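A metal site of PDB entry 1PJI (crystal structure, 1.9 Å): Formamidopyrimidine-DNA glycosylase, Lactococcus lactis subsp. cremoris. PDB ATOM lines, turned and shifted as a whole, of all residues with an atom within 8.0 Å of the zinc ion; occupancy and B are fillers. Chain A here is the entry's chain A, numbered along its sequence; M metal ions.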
ATOM      1  N   TRP A 179       3.911 -26.202  -0.424  1.00  0.00           N
ATOM      2  CA  TRP A 179       4.281 -27.157  -1.463  1.00  0.00           C
ATOM      3  C   TRP A 179       5.150 -28.240  -0.834  1.00  0.00           C
ATOM      4  O   TRP A 179       4.991 -29.422  -1.119  1.00  0.00           O
ATOM      5  CB  TRP A 179       5.055 -26.478  -2.585  1.00  0.00           C
ATOM      6  CG  TRP A 179       5.572 -27.448  -3.629  1.00  0.00           C
ATOM      7  CD1 TRP A 179       4.916 -27.879  -4.756  1.00  0.00           C
ATOM      8  CD2 TRP A 179       6.854 -28.099  -3.635  1.00  0.00           C
ATOM      9  NE1 TRP A 179       5.718 -28.749  -5.459  1.00  0.00           N
ATOM     10  CE2 TRP A 179       6.908 -28.910  -4.792  1.00  0.00           C
ATOM     11  CE3 TRP A 179       7.955 -28.078  -2.766  1.00  0.00           C
ATOM     12  CZ2 TRP A 179       8.024 -29.679  -5.115  1.00  0.00           C
ATOM     13  CZ3 TRP A 179       9.068 -28.854  -3.082  1.00  0.00           C
ATOM     14  CH2 TRP A 179       9.085 -29.650  -4.252  1.00  0.00           C
ATOM     15  N   LYS A 182       3.032 -30.494   1.131  1.00  0.00           N
ATOM     16  CA  LYS A 182       1.964 -31.080   0.334  1.00  0.00           C
ATOM     17  C   LYS A 182       0.561 -30.738   0.826  1.00  0.00           C
ATOM     18  O   LYS A 182      -0.300 -31.607   0.942  1.00  0.00           O
ATOM     19  CB  LYS A 182       2.144 -32.605   0.272  1.00  0.00           C
ATOM     20  CG  LYS A 182       3.487 -33.034  -0.306  1.00  0.00           C
ATOM     21  CD  LYS A 182       3.664 -34.545  -0.259  1.00  0.00           C
ATOM     22  CE  LYS A 182       5.047 -34.950  -0.760  1.00  0.00           C
ATOM     23  NZ  LYS A 182       5.301 -36.416  -0.618  1.00  0.00           N
ATOM     24  N   VAL A 237       8.046 -23.371  -6.273  1.00  0.00           N
ATOM     25  CA  VAL A 237       6.765 -22.980  -6.861  1.00  0.00           C
ATOM     26  C   VAL A 237       6.492 -21.487  -7.041  1.00  0.00           C
ATOM     27  O   VAL A 237       5.882 -21.088  -8.030  1.00  0.00           O
ATOM     28  CB  VAL A 237       5.581 -23.566  -6.060  1.00  0.00           C
ATOM     29  CG1 VAL A 237       5.548 -25.067  -6.242  1.00  0.00           C
ATOM     30  CG2 VAL A 237       5.713 -23.204  -4.577  1.00  0.00           C
ATOM     31  N   LYS A 244       7.215 -27.205 -14.624  1.00  0.00           N
ATOM     32  CA  LYS A 244       6.892 -28.537 -14.101  1.00  0.00           C
ATOM     33  C   LYS A 244       7.393 -28.774 -12.684  1.00  0.00           C
ATOM     34  O   LYS A 244       8.551 -28.481 -12.369  1.00  0.00           O
ATOM     35  CB  LYS A 244       7.466 -29.609 -15.036  1.00  0.00           C
ATOM     36  CG  LYS A 244       7.184 -29.402 -16.517  1.00  0.00           C
ATOM     37  CD  LYS A 244       5.690 -29.386 -16.835  1.00  0.00           C
ATOM     38  CE  LYS A 244       5.468 -29.256 -18.349  1.00  0.00           C
ATOM     39  NZ  LYS A 244       4.026 -29.290 -18.737  1.00  0.00           N
ATOM     40  N   CYS A 245       6.514 -29.310 -11.844  1.00  0.00           N
ATOM     41  CA  CYS A 245       6.856 -29.619 -10.463  1.00  0.00           C
ATOM     42  C   CYS A 245       8.040 -30.567 -10.423  1.00  0.00           C
ATOM     43  O   CYS A 245       8.097 -31.542 -11.171  1.00  0.00           O
ATOM     44  CB  CYS A 245       5.653 -30.276  -9.773  1.00  0.00           C
ATOM     45  SG  CYS A 245       6.003 -30.901  -8.118  1.00  0.00           S
ATOM     46  N   SER A 246       8.997 -30.289  -9.538  1.00  0.00           N
ATOM     47  CA  SER A 246      10.201 -31.118  -9.413  1.00  0.00           C
ATOM     48  C   SER A 246       9.954 -32.491  -8.804  1.00  0.00           C
ATOM     49  O   SER A 246      10.844 -33.341  -8.819  1.00  0.00           O
ATOM     50  CB  SER A 246      11.239 -30.379  -8.572  1.00  0.00           C
ATOM     51  OG  SER A 246      10.747 -30.180  -7.255  1.00  0.00           O
ATOM     52  N   ARG A 247       8.752 -32.725  -8.275  1.00  0.00           N
ATOM     53  CA  ARG A 247       8.439 -34.024  -7.678  1.00  0.00           C
ATOM     54  C   ARG A 247       7.586 -34.925  -8.560  1.00  0.00           C
ATOM     55  O   ARG A 247       7.833 -36.121  -8.635  1.00  0.00           O
ATOM     56  CB  ARG A 247       7.727 -33.847  -6.332  1.00  0.00           C
ATOM     57  CG  ARG A 247       8.649 -33.498  -5.159  1.00  0.00           C
ATOM     58  CD  ARG A 247       7.889 -33.455  -3.839  1.00  0.00           C
ATOM     59  NE  ARG A 247       6.707 -32.596  -3.930  1.00  0.00           N
ATOM     60  CZ  ARG A 247       6.202 -31.898  -2.920  1.00  0.00           C
ATOM     61  NH1 ARG A 247       6.768 -31.941  -1.722  1.00  0.00           N
ATOM     62  NH2 ARG A 247       5.123 -31.144  -3.112  1.00  0.00           N
ATOM     63  N   CYS A 248       6.588 -34.349  -9.231  1.00  0.00           N
ATOM     64  CA  CYS A 248       5.698 -35.165 -10.050  1.00  0.00           C
ATOM     65  C   CYS A 248       5.621 -34.813 -11.537  1.00  0.00           C
ATOM     66  O   CYS A 248       5.067 -35.581 -12.322  1.00  0.00           O
ATOM     67  CB  CYS A 248       4.298 -35.122  -9.465  1.00  0.00           C
ATOM     68  SG  CYS A 248       3.431 -33.595  -9.818  1.00  0.00           S
ATOM     69  N   GLY A 249       6.136 -33.645 -11.920  1.00  0.00           N
ATOM     70  CA  GLY A 249       6.095 -33.254 -13.318  1.00  0.00           C
ATOM     71  C   GLY A 249       4.876 -32.467 -13.764  1.00  0.00           C
ATOM     72  O   GLY A 249       4.827 -31.971 -14.890  1.00  0.00           O
ATOM     73  N   ALA A 250       3.874 -32.341 -12.898  1.00  0.00           N
ATOM     74  CA  ALA A 250       2.678 -31.585 -13.252  1.00  0.00           C
ATOM     75  C   ALA A 250       3.034 -30.097 -13.332  1.00  0.00           C
ATOM     76  O   ALA A 250       3.980 -29.658 -12.695  1.00  0.00           O
ATOM     77  CB  ALA A 250       1.589 -31.805 -12.214  1.00  0.00           C
ATOM     78  N   GLU A 251       2.273 -29.334 -14.101  1.00  0.00           N
ATOM     79  CA  GLU A 251       2.525 -27.901 -14.224  1.00  0.00           C
ATOM     80  C   GLU A 251       2.034 -27.113 -13.016  1.00  0.00           C
ATOM     81  O   GLU A 251       0.908 -27.299 -12.557  1.00  0.00           O
ATOM     82  CB  GLU A 251       1.856 -27.317 -15.470  1.00  0.00           C
ATOM     83  CG  GLU A 251       2.619 -27.536 -16.751  1.00  0.00           C
ATOM     84  CD  GLU A 251       2.203 -26.594 -17.866  1.00  0.00           C
ATOM     85  OE1 GLU A 251       2.759 -26.734 -18.981  1.00  0.00           O
ATOM     86  OE2 GLU A 251       1.341 -25.703 -17.637  1.00  0.00           O
ATOM     87  N   ILE A 252       2.889 -26.231 -12.511  1.00  0.00           N
ATOM     88  CA  ILE A 252       2.530 -25.398 -11.384  1.00  0.00           C
ATOM     89  C   ILE A 252       1.449 -24.421 -11.848  1.00  0.00           C
ATOM     90  O   ILE A 252       1.596 -23.774 -12.881  1.00  0.00           O
ATOM     91  CB  ILE A 252       3.761 -24.600 -10.881  1.00  0.00           C
ATOM     92  CG1 ILE A 252       4.861 -25.566 -10.442  1.00  0.00           C
ATOM     93  CG2 ILE A 252       3.363 -23.659  -9.753  1.00  0.00           C
ATOM     94  CD1 ILE A 252       4.444 -26.571  -9.352  1.00  0.00           C
ATOM     95  N   PHE A 264       1.038 -23.298  -6.727  1.00  0.00           N
ATOM     96  CA  PHE A 264       0.979 -24.633  -6.143  1.00  0.00           C
ATOM     97  C   PHE A 264       0.931 -25.730  -7.204  1.00  0.00           C
ATOM     98  O   PHE A 264       0.592 -25.470  -8.364  1.00  0.00           O
ATOM     99  CB  PHE A 264      -0.264 -24.750  -5.273  1.00  0.00           C
ATOM    100  CG  PHE A 264      -1.550 -24.840  -6.061  1.00  0.00           C
ATOM    101  CD1 PHE A 264      -2.199 -26.051  -6.222  1.00  0.00           C
ATOM    102  CD2 PHE A 264      -2.069 -23.712  -6.696  1.00  0.00           C
ATOM    103  CE1 PHE A 264      -3.363 -26.148  -7.000  1.00  0.00           C
ATOM    104  CE2 PHE A 264      -3.229 -23.788  -7.482  1.00  0.00           C
ATOM    105  CZ  PHE A 264      -3.872 -25.020  -7.632  1.00  0.00           C
ATOM    106  N   CYS A 265       1.281 -26.950  -6.807  1.00  0.00           N
ATOM    107  CA  CYS A 265       1.227 -28.106  -7.686  1.00  0.00           C
ATOM    108  C   CYS A 265      -0.093 -28.825  -7.399  1.00  0.00           C
ATOM    109  O   CYS A 265      -0.316 -29.292  -6.271  1.00  0.00           O
ATOM    110  CB  CYS A 265       2.382 -29.072  -7.424  1.00  0.00           C
ATOM    111  SG  CYS A 265       2.176 -30.686  -8.267  1.00  0.00           S
ATOM    112  N   PRO A 266      -0.978 -28.916  -8.396  1.00  0.00           N
ATOM    113  CA  PRO A 266      -2.290 -29.563  -8.291  1.00  0.00           C
ATOM    114  C   PRO A 266      -2.252 -31.036  -7.896  1.00  0.00           C
ATOM    115  O   PRO A 266      -3.230 -31.567  -7.377  1.00  0.00           O
ATOM    116  CB  PRO A 266      -2.879 -29.377  -9.701  1.00  0.00           C
ATOM    117  CG  PRO A 266      -2.209 -28.155 -10.203  1.00  0.00           C
ATOM    118  CD  PRO A 266      -0.786 -28.363  -9.749  1.00  0.00           C
ATOM    119  N   VAL A 267      -1.131 -31.695  -8.160  1.00  0.00           N
ATOM    120  CA  VAL A 267      -0.986 -33.114  -7.833  1.00  0.00           C
ATOM    121  C   VAL A 267      -0.455 -33.324  -6.409  1.00  0.00           C
ATOM    122  O   VAL A 267      -1.030 -34.086  -5.626  1.00  0.00           O
ATOM    123  CB  VAL A 267      -0.024 -33.814  -8.827  1.00  0.00           C
ATOM    124  CG1 VAL A 267       0.231 -35.238  -8.383  1.00  0.00           C
ATOM    125  CG2 VAL A 267      -0.629 -33.791 -10.236  1.00  0.00           C
ATOM    126  N   CYS A 268       0.647 -32.665  -6.076  1.00  0.00           N
ATOM    127  CA  CYS A 268       1.256 -32.794  -4.760  1.00  0.00           C
ATOM    128  C   CYS A 268       0.419 -32.137  -3.664  1.00  0.00           C
ATOM    129  O   CYS A 268       0.491 -32.539  -2.501  1.00  0.00           O
ATOM    130  CB  CYS A 268       2.656 -32.174  -4.776  1.00  0.00           C
ATOM    131  SG  CYS A 268       3.886 -33.071  -5.744  1.00  0.00           S
ATOM    132  N   GLN A 269      -0.375 -31.141  -4.039  1.00  0.00           N
ATOM    133  CA  GLN A 269      -1.216 -30.415  -3.092  1.00  0.00           C
ATOM    134  C   GLN A 269      -2.693 -30.600  -3.418  1.00  0.00           C
ATOM    135  O   GLN A 269      -3.336 -29.716  -3.982  1.00  0.00           O
ATOM    136  CB  GLN A 269      -0.837 -28.932  -3.112  1.00  0.00           C
ATOM    137  CG  GLN A 269       0.572 -28.658  -2.561  1.00  0.00           C
ATOM    138  CD  GLN A 269       1.089 -27.267  -2.895  1.00  0.00           C
ATOM    139  OE1 GLN A 269       1.707 -27.058  -3.938  1.00  0.00           O
ATOM    140  NE2 GLN A 269       0.820 -26.307  -2.011  1.00  0.00           N
HETATM  141 ZN    ZN M   1       3.867 -32.029  -7.910  1.00  0.00          ZN
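The side-chain sulfur (SG) of Cys 265 sits close to the backbone NH (N) of Val 267, 3.5 Å away. The side-chain amide oxygen of Gln 269 is in hydrogen-bond range of the backbone NH of Cys 265, 2.9 Å away. SG of Cys 268 sits close to NE of Arg 247 (3.4 Å). The side-chain sulfur of Cys 245 lies close to the indole nitrogen of Trp 179, 3.4 Å away. The backbone NH (N) of Arg 247 lies close to the side-chain sulfur (SG) of Cys 245 (3.3 Å). The backbone NH (N) of Cys 245 sits at hydrogen-bond distance from the backbone carbonyl oxygen (O) of Ala 250 (2.7 Å). The backbone NH of Ala 250 lies close to the side-chain sulfur of Cys 248.
Four residues have an atom within 4 Å of the zinc ion: Cys 245, Cys 248, Cys 265 and Cys 268.
The zinc ion is bound by SG of Cys 265 (2.2 Å), SG of Cys 268 (2.4 Å), SG of Cys 245 (2.4 Å) and SG of Cys 248 (2.5 Å). The zinc ion has four donor atoms within binding distance.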
